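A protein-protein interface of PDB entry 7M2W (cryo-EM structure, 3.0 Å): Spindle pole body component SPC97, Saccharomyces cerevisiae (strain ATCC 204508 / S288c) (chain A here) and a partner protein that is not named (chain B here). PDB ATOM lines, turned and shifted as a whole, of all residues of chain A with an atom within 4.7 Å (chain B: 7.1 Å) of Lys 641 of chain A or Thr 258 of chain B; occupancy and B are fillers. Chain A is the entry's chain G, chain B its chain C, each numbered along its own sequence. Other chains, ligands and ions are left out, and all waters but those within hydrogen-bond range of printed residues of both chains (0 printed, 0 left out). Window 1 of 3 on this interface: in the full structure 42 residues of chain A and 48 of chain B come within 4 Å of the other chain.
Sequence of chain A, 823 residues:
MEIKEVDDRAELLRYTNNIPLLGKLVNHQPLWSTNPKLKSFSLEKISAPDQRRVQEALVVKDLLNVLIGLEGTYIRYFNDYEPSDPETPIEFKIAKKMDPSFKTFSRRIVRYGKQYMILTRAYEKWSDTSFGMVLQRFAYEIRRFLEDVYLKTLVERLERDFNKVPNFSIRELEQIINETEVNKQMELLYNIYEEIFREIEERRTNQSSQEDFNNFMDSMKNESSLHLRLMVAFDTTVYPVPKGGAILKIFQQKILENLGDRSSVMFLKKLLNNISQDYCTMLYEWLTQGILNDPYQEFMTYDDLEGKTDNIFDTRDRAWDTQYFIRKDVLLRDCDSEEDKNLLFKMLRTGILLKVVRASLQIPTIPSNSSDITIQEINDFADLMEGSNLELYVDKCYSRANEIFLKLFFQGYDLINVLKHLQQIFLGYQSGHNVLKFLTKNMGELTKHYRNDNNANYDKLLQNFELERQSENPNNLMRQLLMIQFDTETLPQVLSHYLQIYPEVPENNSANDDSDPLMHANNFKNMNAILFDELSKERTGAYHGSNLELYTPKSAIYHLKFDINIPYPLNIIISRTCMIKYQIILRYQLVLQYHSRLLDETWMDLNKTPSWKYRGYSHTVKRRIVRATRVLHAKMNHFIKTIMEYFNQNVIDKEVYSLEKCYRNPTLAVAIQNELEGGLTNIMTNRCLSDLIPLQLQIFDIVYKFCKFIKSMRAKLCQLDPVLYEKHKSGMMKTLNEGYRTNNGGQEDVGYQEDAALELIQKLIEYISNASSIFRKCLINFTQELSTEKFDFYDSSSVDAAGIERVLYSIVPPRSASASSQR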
ATOM      1  N   SER A 596      -6.939 -11.192  -1.584  1.00  0.00           N
ATOM      2  CA  SER A 596      -7.830 -11.384  -0.445  1.00  0.00           C
ATOM      3  C   SER A 596      -8.145 -12.857  -0.234  1.00  0.00           C
ATOM      4  O   SER A 596      -8.205 -13.314   0.909  1.00  0.00           O
ATOM      5  CB  SER A 596      -9.122 -10.597  -0.633  1.00  0.00           C
ATOM      6  OG  SER A 596      -9.907 -11.157  -1.667  1.00  0.00           O
ATOM      7  N   ASP A 600      -7.373 -15.109   2.968  1.00  0.00           N
ATOM      8  CA  ASP A 600      -8.429 -15.947   3.529  1.00  0.00           C
ATOM      9  C   ASP A 600      -7.948 -17.375   3.742  1.00  0.00           C
ATOM     10  O   ASP A 600      -8.064 -17.917   4.847  1.00  0.00           O
ATOM     11  CB  ASP A 600      -9.650 -15.942   2.614  1.00  0.00           C
ATOM     12  CG  ASP A 600     -10.411 -14.639   2.654  1.00  0.00           C
ATOM     13  OD1 ASP A 600     -11.611 -14.658   2.318  1.00  0.00           O
ATOM     14  OD2 ASP A 600      -9.824 -13.607   3.040  1.00  0.00           O
ATOM     15  N   ASN A 637      -3.940  -8.609   6.150  1.00  0.00           N
ATOM     16  CA  ASN A 637      -5.361  -8.807   5.905  1.00  0.00           C
ATOM     17  C   ASN A 637      -6.125  -7.506   6.063  1.00  0.00           C
ATOM     18  O   ASN A 637      -6.960  -7.163   5.224  1.00  0.00           O
ATOM     19  CB  ASN A 637      -5.906  -9.872   6.853  1.00  0.00           C
ATOM     20  CG  ASN A 637      -7.271 -10.377   6.444  1.00  0.00           C
ATOM     21  OD1 ASN A 637      -7.446 -10.906   5.349  1.00  0.00           O
ATOM     22  ND2 ASN A 637      -8.246 -10.225   7.330  1.00  0.00           N
ATOM     23  N   HIS A 638      -5.845  -6.761   7.130  1.00  0.00           N
ATOM     24  CA  HIS A 638      -6.534  -5.495   7.337  1.00  0.00           C
ATOM     25  C   HIS A 638      -6.235  -4.521   6.207  1.00  0.00           C
ATOM     26  O   HIS A 638      -7.149  -3.875   5.687  1.00  0.00           O
ATOM     27  CB  HIS A 638      -6.149  -4.907   8.693  1.00  0.00           C
ATOM     28  CG  HIS A 638      -6.684  -5.685   9.857  1.00  0.00           C
ATOM     29  ND1 HIS A 638      -7.857  -6.405   9.794  1.00  0.00           N
ATOM     30  CD2 HIS A 638      -6.202  -5.860  11.109  1.00  0.00           C
ATOM     31  CE1 HIS A 638      -8.078  -6.987  10.960  1.00  0.00           C
ATOM     32  NE2 HIS A 638      -7.087  -6.673  11.775  1.00  0.00           N
ATOM     33  N   PHE A 639      -4.973  -4.438   5.776  1.00  0.00           N
ATOM     34  CA  PHE A 639      -4.626  -3.539   4.677  1.00  0.00           C
ATOM     35  C   PHE A 639      -5.351  -3.927   3.395  1.00  0.00           C
ATOM     36  O   PHE A 639      -5.968  -3.082   2.742  1.00  0.00           O
ATOM     37  CB  PHE A 639      -3.116  -3.534   4.447  1.00  0.00           C
ATOM     38  CG  PHE A 639      -2.703  -2.865   3.164  1.00  0.00           C
ATOM     39  CD1 PHE A 639      -2.561  -1.490   3.103  1.00  0.00           C
ATOM     40  CD2 PHE A 639      -2.465  -3.607   2.020  1.00  0.00           C
ATOM     41  CE1 PHE A 639      -2.186  -0.867   1.929  1.00  0.00           C
ATOM     42  CE2 PHE A 639      -2.095  -2.988   0.841  1.00  0.00           C
ATOM     43  CZ  PHE A 639      -1.953  -1.618   0.798  1.00  0.00           C
ATOM     44  N   ILE A 640      -5.247  -5.197   2.995  1.00  0.00           N
ATOM     45  CA  ILE A 640      -5.867  -5.638   1.747  1.00  0.00           C
ATOM     46  C   ILE A 640      -7.373  -5.436   1.791  1.00  0.00           C
ATOM     47  O   ILE A 640      -7.966  -4.878   0.858  1.00  0.00           O
ATOM     48  CB  ILE A 640      -5.499  -7.103   1.448  1.00  0.00           C
ATOM     49  CG1 ILE A 640      -3.996  -7.236   1.220  1.00  0.00           C
ATOM     50  CG2 ILE A 640      -6.258  -7.600   0.236  1.00  0.00           C
ATOM     51  CD1 ILE A 640      -3.496  -6.444   0.033  1.00  0.00           C
ATOM     52  N   LYS A 641      -8.021  -5.894   2.864  1.00  0.00           N
ATOM     53  CA  LYS A 641      -9.470  -5.771   2.956  1.00  0.00           C
ATOM     54  C   LYS A 641      -9.899  -4.312   3.010  1.00  0.00           C
ATOM     55  O   LYS A 641     -10.954  -3.961   2.481  1.00  0.00           O
ATOM     56  CB  LYS A 641      -9.992  -6.525   4.177  1.00  0.00           C
ATOM     57  CG  LYS A 641      -9.690  -8.012   4.180  1.00  0.00           C
ATOM     58  CD  LYS A 641     -10.055  -8.660   2.865  1.00  0.00           C
ATOM     59  CE  LYS A 641      -9.946 -10.169   2.960  1.00  0.00           C
ATOM     60  NZ  LYS A 641     -10.933 -10.730   3.917  1.00  0.00           N
ATOM     61  N   THR A 642      -9.077  -3.437   3.593  1.00  0.00           N
ATOM     62  CA  THR A 642      -9.450  -2.031   3.676  1.00  0.00           C
ATOM     63  C   THR A 642      -9.281  -1.340   2.331  1.00  0.00           C
ATOM     64  O   THR A 642     -10.103  -0.507   1.941  1.00  0.00           O
ATOM     65  CB  THR A 642      -8.620  -1.332   4.750  1.00  0.00           C
ATOM     66  OG1 THR A 642      -8.872  -1.944   6.020  1.00  0.00           O
ATOM     67  CG2 THR A 642      -8.982   0.139   4.823  1.00  0.00           C
ATOM     68  N   ILE A 643      -8.212  -1.671   1.607  1.00  0.00           N
ATOM     69  CA  ILE A 643      -8.046  -1.150   0.255  1.00  0.00           C
ATOM     70  C   ILE A 643      -9.208  -1.588  -0.623  1.00  0.00           C
ATOM     71  O   ILE A 643      -9.780  -0.786  -1.372  1.00  0.00           O
ATOM     72  CB  ILE A 643      -6.696  -1.601  -0.329  1.00  0.00           C
ATOM     73  CG1 ILE A 643      -5.556  -0.800   0.294  1.00  0.00           C
ATOM     74  CG2 ILE A 643      -6.684  -1.439  -1.834  1.00  0.00           C
ATOM     75  CD1 ILE A 643      -5.668   0.687   0.064  1.00  0.00           C
ATOM     76  N   MET A 644      -9.583  -2.865  -0.534  1.00  0.00           N
ATOM     77  CA  MET A 644     -10.690  -3.366  -1.338  1.00  0.00           C
ATOM     78  C   MET A 644     -12.010  -2.725  -0.927  1.00  0.00           C
ATOM     79  O   MET A 644     -12.836  -2.398  -1.783  1.00  0.00           O
ATOM     80  CB  MET A 644     -10.770  -4.886  -1.228  1.00  0.00           C
ATOM     81  CG  MET A 644      -9.626  -5.621  -1.876  1.00  0.00           C
ATOM     82  SD  MET A 644      -9.909  -7.395  -1.852  1.00  0.00           S
ATOM     83  CE  MET A 644     -11.612  -7.469  -2.394  1.00  0.00           C
ATOM     84  N   GLU A 645     -12.227  -2.537   0.376  1.00  0.00           N
ATOM     85  CA  GLU A 645     -13.425  -1.846   0.839  1.00  0.00           C
ATOM     86  C   GLU A 645     -13.486  -0.432   0.288  1.00  0.00           C
ATOM     87  O   GLU A 645     -14.500  -0.028  -0.291  1.00  0.00           O
ATOM     88  CB  GLU A 645     -13.460  -1.816   2.365  1.00  0.00           C
ATOM     89  CG  GLU A 645     -13.944  -3.093   3.015  1.00  0.00           C
ATOM     90  CD  GLU A 645     -13.823  -3.049   4.523  1.00  0.00           C
ATOM     91  OE1 GLU A 645     -13.529  -1.962   5.061  1.00  0.00           O
ATOM     92  OE2 GLU A 645     -14.013  -4.100   5.169  1.00  0.00           O
ATOM     93  N   MET B 248     -17.357  -7.410  -1.749  1.00  0.00           N
ATOM     94  CA  MET B 248     -16.248  -7.688  -0.841  1.00  0.00           C
ATOM     95  C   MET B 248     -16.223  -9.096  -0.257  1.00  0.00           C
ATOM     96  O   MET B 248     -15.271  -9.840  -0.505  1.00  0.00           O
ATOM     97  CB  MET B 248     -16.271  -6.689   0.317  1.00  0.00           C
ATOM     98  CG  MET B 248     -15.706  -5.340  -0.022  1.00  0.00           C
ATOM     99  SD  MET B 248     -13.918  -5.416  -0.088  1.00  0.00           S
ATOM    100  CE  MET B 248     -13.557  -6.331   1.405  1.00  0.00           C
ATOM    101  N   TYR B 249     -17.241  -9.491   0.511  1.00  0.00           N
ATOM    102  CA  TYR B 249     -17.131 -10.631   1.433  1.00  0.00           C
ATOM    103  C   TYR B 249     -18.073 -11.747   0.993  1.00  0.00           C
ATOM    104  O   TYR B 249     -19.233 -11.789   1.404  1.00  0.00           O
ATOM    105  CB  TYR B 249     -17.421 -10.190   2.861  1.00  0.00           C
ATOM    106  CG  TYR B 249     -16.424  -9.215   3.437  1.00  0.00           C
ATOM    107  CD1 TYR B 249     -16.814  -7.943   3.822  1.00  0.00           C
ATOM    108  CD2 TYR B 249     -15.095  -9.567   3.603  1.00  0.00           C
ATOM    109  CE1 TYR B 249     -15.911  -7.050   4.352  1.00  0.00           C
ATOM    110  CE2 TYR B 249     -14.183  -8.680   4.132  1.00  0.00           C
ATOM    111  CZ  TYR B 249     -14.599  -7.424   4.507  1.00  0.00           C
ATOM    112  OH  TYR B 249     -13.694  -6.535   5.033  1.00  0.00           O
ATOM    113  N   SER B 251     -17.506 -15.022   1.604  1.00  0.00           N
ATOM    114  CA  SER B 251     -17.248 -16.224   2.382  1.00  0.00           C
ATOM    115  C   SER B 251     -17.044 -15.862   3.843  1.00  0.00           C
ATOM    116  O   SER B 251     -16.455 -14.828   4.165  1.00  0.00           O
ATOM    117  CB  SER B 251     -16.021 -16.980   1.866  1.00  0.00           C
ATOM    118  OG  SER B 251     -15.979 -18.292   2.393  1.00  0.00           O
ATOM    119  N   MET B 252     -17.542 -16.731   4.727  1.00  0.00           N
ATOM    120  CA  MET B 252     -17.302 -16.566   6.156  1.00  0.00           C
ATOM    121  C   MET B 252     -15.818 -16.551   6.485  1.00  0.00           C
ATOM    122  O   MET B 252     -15.426 -15.973   7.505  1.00  0.00           O
ATOM    123  CB  MET B 252     -17.995 -17.680   6.941  1.00  0.00           C
ATOM    124  CG  MET B 252     -19.469 -17.854   6.622  1.00  0.00           C
ATOM    125  SD  MET B 252     -20.487 -16.490   7.214  1.00  0.00           S
ATOM    126  CE  MET B 252     -20.515 -16.829   8.968  1.00  0.00           C
ATOM    127  N   SER B 253     -14.992 -17.184   5.649  1.00  0.00           N
ATOM    128  CA  SER B 253     -13.548 -17.099   5.804  1.00  0.00           C
ATOM    129  C   SER B 253     -13.061 -15.658   5.839  1.00  0.00           C
ATOM    130  O   SER B 253     -12.273 -15.309   6.721  1.00  0.00           O
ATOM    131  CB  SER B 253     -12.854 -17.853   4.670  1.00  0.00           C
ATOM    132  OG  SER B 253     -12.904 -19.252   4.885  1.00  0.00           O
ATOM    133  N   SER B 254     -13.527 -14.816   4.915  1.00  0.00           N
ATOM    134  CA  SER B 254     -13.120 -13.416   4.889  1.00  0.00           C
ATOM    135  C   SER B 254     -13.605 -12.674   6.127  1.00  0.00           C
ATOM    136  O   SER B 254     -12.836 -11.940   6.761  1.00  0.00           O
ATOM    137  CB  SER B 254     -13.652 -12.744   3.627  1.00  0.00           C
ATOM    138  OG  SER B 254     -15.068 -12.711   3.639  1.00  0.00           O
ATOM    139  N   ILE B 255     -14.883 -12.848   6.472  1.00  0.00           N
ATOM    140  CA  ILE B 255     -15.441 -12.227   7.670  1.00  0.00           C
ATOM    141  C   ILE B 255     -14.573 -12.530   8.881  1.00  0.00           C
ATOM    142  O   ILE B 255     -14.137 -11.622   9.598  1.00  0.00           O
ATOM    143  CB  ILE B 255     -16.884 -12.708   7.893  1.00  0.00           C
ATOM    144  CG1 ILE B 255     -17.708 -12.552   6.618  1.00  0.00           C
ATOM    145  CG2 ILE B 255     -17.522 -11.941   9.033  1.00  0.00           C
ATOM    146  CD1 ILE B 255     -17.968 -11.140   6.247  1.00  0.00           C
ATOM    147  N   TYR B 256     -14.310 -13.811   9.130  1.00  0.00           N
ATOM    148  CA  TYR B 256     -13.602 -14.194  10.343  1.00  0.00           C
ATOM    149  C   TYR B 256     -12.127 -13.813  10.293  1.00  0.00           C
ATOM    150  O   TYR B 256     -11.578 -13.363  11.305  1.00  0.00           O
ATOM    151  CB  TYR B 256     -13.794 -15.686  10.588  1.00  0.00           C
ATOM    152  CG  TYR B 256     -15.228 -16.010  10.921  1.00  0.00           C
ATOM    153  CD1 TYR B 256     -15.787 -17.234  10.584  1.00  0.00           C
ATOM    154  CD2 TYR B 256     -16.027 -15.083  11.576  1.00  0.00           C
ATOM    155  CE1 TYR B 256     -17.102 -17.519  10.889  1.00  0.00           C
ATOM    156  CE2 TYR B 256     -17.337 -15.362  11.886  1.00  0.00           C
ATOM    157  CZ  TYR B 256     -17.871 -16.579  11.542  1.00  0.00           C
ATOM    158  OH  TYR B 256     -19.179 -16.852  11.855  1.00  0.00           O
ATOM    159  N   SER B 257     -11.465 -13.987   9.144  1.00  0.00           N
ATOM    160  CA  SER B 257     -10.106 -13.481   8.992  1.00  0.00           C
ATOM    161  C   SER B 257     -10.030 -12.001   9.328  1.00  0.00           C
ATOM    162  O   SER B 257      -9.026 -11.537   9.882  1.00  0.00           O
ATOM    163  CB  SER B 257      -9.612 -13.722   7.569  1.00  0.00           C
ATOM    164  OG  SER B 257     -10.363 -12.956   6.646  1.00  0.00           O
ATOM    165  N   THR B 258     -11.077 -11.248   9.001  1.00  0.00           N
ATOM    166  CA  THR B 258     -11.160  -9.864   9.446  1.00  0.00           C
ATOM    167  C   THR B 258     -11.363  -9.789  10.954  1.00  0.00           C
ATOM    168  O   THR B 258     -10.826  -8.900  11.623  1.00  0.00           O
ATOM    169  CB  THR B 258     -12.299  -9.160   8.711  1.00  0.00           C
ATOM    170  OG1 THR B 258     -12.015  -9.124   7.309  1.00  0.00           O
ATOM    171  CG2 THR B 258     -12.484  -7.761   9.233  1.00  0.00           C
ATOM    172  N   LEU B 259     -12.121 -10.733  11.506  1.00  0.00           N
ATOM    173  CA  LEU B 259     -12.552 -10.666  12.896  1.00  0.00           C
ATOM    174  C   LEU B 259     -11.640 -11.404  13.866  1.00  0.00           C
ATOM    175  O   LEU B 259     -11.590 -11.036  15.044  1.00  0.00           O
ATOM    176  CB  LEU B 259     -13.966 -11.233  13.023  1.00  0.00           C
ATOM    177  CG  LEU B 259     -15.085 -10.220  12.830  1.00  0.00           C
ATOM    178  CD1 LEU B 259     -16.412 -10.923  12.661  1.00  0.00           C
ATOM    179  CD2 LEU B 259     -15.112  -9.309  14.023  1.00  0.00           C
ATOM    180  N   ILE B 260     -10.924 -12.428  13.416  1.00  0.00           N
ATOM    181  CA  ILE B 260     -10.226 -13.318  14.338  1.00  0.00           C
ATOM    182  C   ILE B 260      -8.722 -13.248  14.101  1.00  0.00           C
ATOM    183  O   ILE B 260      -8.233 -13.724  13.067  1.00  0.00           O
ATOM    184  CB  ILE B 260     -10.740 -14.757  14.197  1.00  0.00           C
ATOM    185  CG1 ILE B 260     -12.174 -14.846  14.712  1.00  0.00           C
ATOM    186  CG2 ILE B 260      -9.847 -15.718  14.956  1.00  0.00           C
ATOM    187  CD1 ILE B 260     -12.818 -16.175  14.455  1.00  0.00           C
ATOM    188  N   PRO B 261      -7.956 -12.661  15.021  1.00  0.00           N
ATOM    189  CA  PRO B 261      -6.497 -12.632  14.845  1.00  0.00           C
ATOM    190  C   PRO B 261      -5.845 -13.998  14.962  1.00  0.00           C
ATOM    191  O   PRO B 261      -5.056 -14.377  14.087  1.00  0.00           O
ATOM    192  CB  PRO B 261      -6.024 -11.688  15.961  1.00  0.00           C
ATOM    193  CG  PRO B 261      -7.264 -11.017  16.478  1.00  0.00           C
ATOM    194  CD  PRO B 261      -8.381 -11.968  16.246  1.00  0.00           C
ATOM    195  N   PHE B 316     -10.398  -5.551  19.851  1.00  0.00           N
ATOM    196  CA  PHE B 316      -9.280  -6.025  19.047  1.00  0.00           C
ATOM    197  C   PHE B 316      -9.633  -5.953  17.568  1.00  0.00           C
ATOM    198  O   PHE B 316      -8.917  -5.326  16.780  1.00  0.00           O
ATOM    199  CB  PHE B 316      -8.895  -7.451  19.446  1.00  0.00           C
ATOM    200  CG  PHE B 316      -8.553  -7.599  20.899  1.00  0.00           C
ATOM    201  CD1 PHE B 316      -9.255  -8.474  21.705  1.00  0.00           C
ATOM    202  CD2 PHE B 316      -7.530  -6.857  21.457  1.00  0.00           C
ATOM    203  CE1 PHE B 316      -8.941  -8.609  23.042  1.00  0.00           C
ATOM    204  CE2 PHE B 316      -7.211  -6.987  22.791  1.00  0.00           C
ATOM    205  CZ  PHE B 316      -7.917  -7.863  23.585  1.00  0.00           C
ATOM    206  N   ASN B 317     -10.734  -6.590  17.184  1.00  0.00           N
ATOM    207  CA  ASN B 317     -11.230  -6.502  15.819  1.00  0.00           C
ATOM    208  C   ASN B 317     -12.673  -6.021  15.817  1.00  0.00           C
ATOM    209  O   ASN B 317     -13.450  -6.339  16.720  1.00  0.00           O
ATOM    210  CB  ASN B 317     -11.137  -7.858  15.119  1.00  0.00           C
ATOM    211  CG  ASN B 317      -9.710  -8.278  14.838  1.00  0.00           C
ATOM    212  OD1 ASN B 317      -8.797  -7.980  15.604  1.00  0.00           O
ATOM    213  ND2 ASN B 317      -9.511  -8.978  13.728  1.00  0.00           N
ATOM    214  N   VAL B 318     -13.026  -5.243  14.799  1.00  0.00           N
ATOM    215  CA  VAL B 318     -14.384  -4.750  14.608  1.00  0.00           C
ATOM    216  C   VAL B 318     -14.775  -5.006  13.162  1.00  0.00           C
ATOM    217  O   VAL B 318     -13.944  -4.878  12.258  1.00  0.00           O
ATOM    218  CB  VAL B 318     -14.513  -3.251  14.943  1.00  0.00           C
ATOM    219  CG1 VAL B 318     -15.970  -2.852  15.023  1.00  0.00           C
ATOM    220  CG2 VAL B 318     -13.812  -2.928  16.247  1.00  0.00           C
ATOM    221  N   TYR B 319     -16.035  -5.369  12.945  1.00  0.00           N
ATOM    222  CA  TYR B 319     -16.577  -5.585  11.613  1.00  0.00           C
ATOM    223  C   TYR B 319     -18.057  -5.236  11.623  1.00  0.00           C
ATOM    224  O   TYR B 319     -18.866  -5.972  12.195  1.00  0.00           O
ATOM    225  CB  TYR B 319     -16.364  -7.028  11.148  1.00  0.00           C
ATOM    226  CG  TYR B 319     -17.179  -7.397   9.930  1.00  0.00           C
ATOM    227  CD1 TYR B 319     -16.748  -7.065   8.656  1.00  0.00           C
ATOM    228  CD2 TYR B 319     -18.377  -8.085  10.055  1.00  0.00           C
ATOM    229  CE1 TYR B 319     -17.491  -7.398   7.543  1.00  0.00           C
ATOM    230  CE2 TYR B 319     -19.124  -8.420   8.949  1.00  0.00           C
ATOM    231  CZ  TYR B 319     -18.678  -8.074   7.696  1.00  0.00           C
ATOM    232  OH  TYR B 319     -19.425  -8.409   6.593  1.00  0.00           O
ATOM    233  N   ALA B 351      -8.198  -0.496  12.505  1.00  0.00           N
ATOM    234  CA  ALA B 351      -9.117  -0.565  11.379  1.00  0.00           C
ATOM    235  C   ALA B 351     -10.459  -1.147  11.802  1.00  0.00           C
ATOM    236  O   ALA B 351     -10.533  -2.245  12.360  1.00  0.00           O
ATOM    237  CB  ALA B 351      -8.514  -1.405  10.254  1.00  0.00           C
ATOM    238  N   MET B 352     -11.522  -0.398  11.534  1.00  0.00           N
ATOM    239  CA  MET B 352     -12.884  -0.892  11.641  1.00  0.00           C
ATOM    240  C   MET B 352     -13.383  -1.204  10.240  1.00  0.00           C
ATOM    241  O   MET B 352     -13.473  -0.313   9.392  1.00  0.00           O
ATOM    242  CB  MET B 352     -13.802   0.135  12.305  1.00  0.00           C
ATOM    243  CG  MET B 352     -13.450   0.449  13.742  1.00  0.00           C
ATOM    244  SD  MET B 352     -13.759   2.178  14.139  1.00  0.00           S
ATOM    245  CE  MET B 352     -12.565   2.977  13.071  1.00  0.00           C
ATOM    246  N   HIS B 353     -13.703  -2.469   9.998  1.00  0.00           N
ATOM    247  CA  HIS B 353     -14.083  -2.936   8.674  1.00  0.00           C
ATOM    248  C   HIS B 353     -15.582  -2.766   8.484  1.00  0.00           C
ATOM    249  O   HIS B 353     -16.376  -3.330   9.241  1.00  0.00           O
ATOM    250  CB  HIS B 353     -13.681  -4.394   8.473  1.00  0.00           C
ATOM    251  CG  HIS B 353     -12.211  -4.591   8.293  1.00  0.00           C
ATOM    252  ND1 HIS B 353     -11.633  -4.787   7.058  1.00  0.00           N
ATOM    253  CD2 HIS B 353     -11.199  -4.623   9.191  1.00  0.00           C
ATOM    254  CE1 HIS B 353     -10.329  -4.931   7.202  1.00  0.00           C
ATOM    255  NE2 HIS B 353     -10.040  -4.837   8.487  1.00  0.00           N
ATOM    256  N   VAL B 354     -15.963  -1.991   7.474  1.00  0.00           N
ATOM    257  CA  VAL B 354     -17.361  -1.709   7.187  1.00  0.00           C
ATOM    258  C   VAL B 354     -17.725  -2.398   5.886  1.00  0.00           C
ATOM    259  O   VAL B 354     -17.259  -1.996   4.814  1.00  0.00           O
ATOM    260  CB  VAL B 354     -17.643  -0.204   7.087  1.00  0.00           C
ATOM    261  CG1 VAL B 354     -19.134   0.037   6.998  1.00  0.00           C
ATOM    262  CG2 VAL B 354     -17.049   0.521   8.272  1.00  0.00           C
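SD of Met 248 of chain B lies within hydrogen-bond range of N of Glu 645 of chain A, at 3.4 Å.
The side-chain hydroxyl (OH) of Tyr 249 of chain B is in hydrogen-bond range of the side-chain carboxylate (OE2) of Glu 645 of chain A (2.5 Å).
The backbone NH (N) of Ser 254 of chain B lies close to the side-chain carboxylate (OD1) of Asp 600 of chain A (3.2 Å).
The side-chain amide nitrogen of Asn 637 of chain A lies within hydrogen-bond range of the backbone carbonyl oxygen of Ser 257 of chain B (3.0 Å).
N of Thr 258 of chain B lies close to ND2 of Asn 637 of chain A (3.4 Å).
A ring nitrogen (ND1) of His 638 of chain A lies within hydrogen-bond range of a ring nitrogen (NE2) of His 353 of chain B (3.0 Å).
The side-chain carboxylate (OE2) of Glu 645 of chain A lies within hydrogen-bond range of a ring nitrogen (ND1) of His 353 of chain B (3.1 Å).
The backbone NH of Val 354 of chain B is in hydrogen-bond range of the side-chain carboxylate of Glu 645 of chain A (3.4 Å).
The backbone carbonyl oxygen (O) of Met 644 of chain A sits close to the side-chain sulfur (SD) of Met 248 of chain B (3.6 Å).
Asp 600 of chain A touches Ser 253 of chain B.
OD2 of Asp 600 of chain A touches OG of Ser 257 of chain B, at 3.7 Å.
O of Thr 258 of chain B touches CE1 of His 638 of chain A, at 3.4 Å.
His 638 of chain A touches Asn 317 of chain B.
Met 248 of chain B touches Lys 641 of chain A.
Lys 641 of chain A touches Tyr 249 of chain B (CB to OH, 3.8 Å).
NZ of Lys 641 of chain A touches CB of Ser 254 of chain B, at 3.4 Å.
Lys 641 of chain A touches Thr 258 of chain B (NZ to OG1, 3.9 Å).
CB of Lys 641 of chain A touches CE1 of His 353 of chain B (3.4 Å).
CE1 of His 353 of chain B touches OG1 of Thr 642 of chain A, at 3.5 Å.
Lys 641 of chain A touches just these residues of chain B: Met 248 (3.7 Å), Tyr 249 (3.8 Å), Ser 254 (3.4 Å), Ser 257 (3.6 Å), Thr 258 (3.9 Å) and His 353 (3.4 Å).
Of chain A, only Asn 637, His 638 and Lys 641 come within 4 Å of Thr 258 of chain B.
Printed residues of chain B within 4 Å of His 638 of chain A: Thr 258 (3.4 Å), Asn 317 (3.7 Å) and His 353 (3.0 Å).
Printed residues of chain A within 4 Å of Val 354 of chain B: Glu 645 (3.4 Å).
Printed residues of chain B within 4 Å of Asn 637 of chain A: Ser 257 and Thr 258.
Of the 21 printed residues of chain B, 9 touch a printed residue of chain A.
Among the printed residues, 20 pairs touch across the chains.
Among the printed residues, no Asp or Glu carboxylate lies within 4 Å of a Lys or Arg side-chain nitrogen of the other chain.
OH of Tyr 249 of chain B is in hydrogen-bond range of ND1 of His 353 of chain B, 3.4 Å away.
O of Thr 258 of chain B is in hydrogen-bond range of ND2 of Asn 317 of chain B.
The backbone carbonyl oxygen of Leu 259 of chain B sits at hydrogen-bond distance from the side-chain amide nitrogen of Asn 317 of chain B (3.2 Å).
The side-chain hydroxyl (OG) of Ser 596 of chain A lies close to the side-chain sulfur (SD) of Met 644 of chain A.
The side-chain amino group (NZ) of Lys 641 of chain A lies within salt-bridge range of the side-chain carboxylate (OD2) of Asp 600 of chain A, 3.2 Å away.
The backbone carbonyl oxygen of His 638 of chain A sits at hydrogen-bond distance from the side-chain hydroxyl of Thr 642 of chain A, at 2.6 Å.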
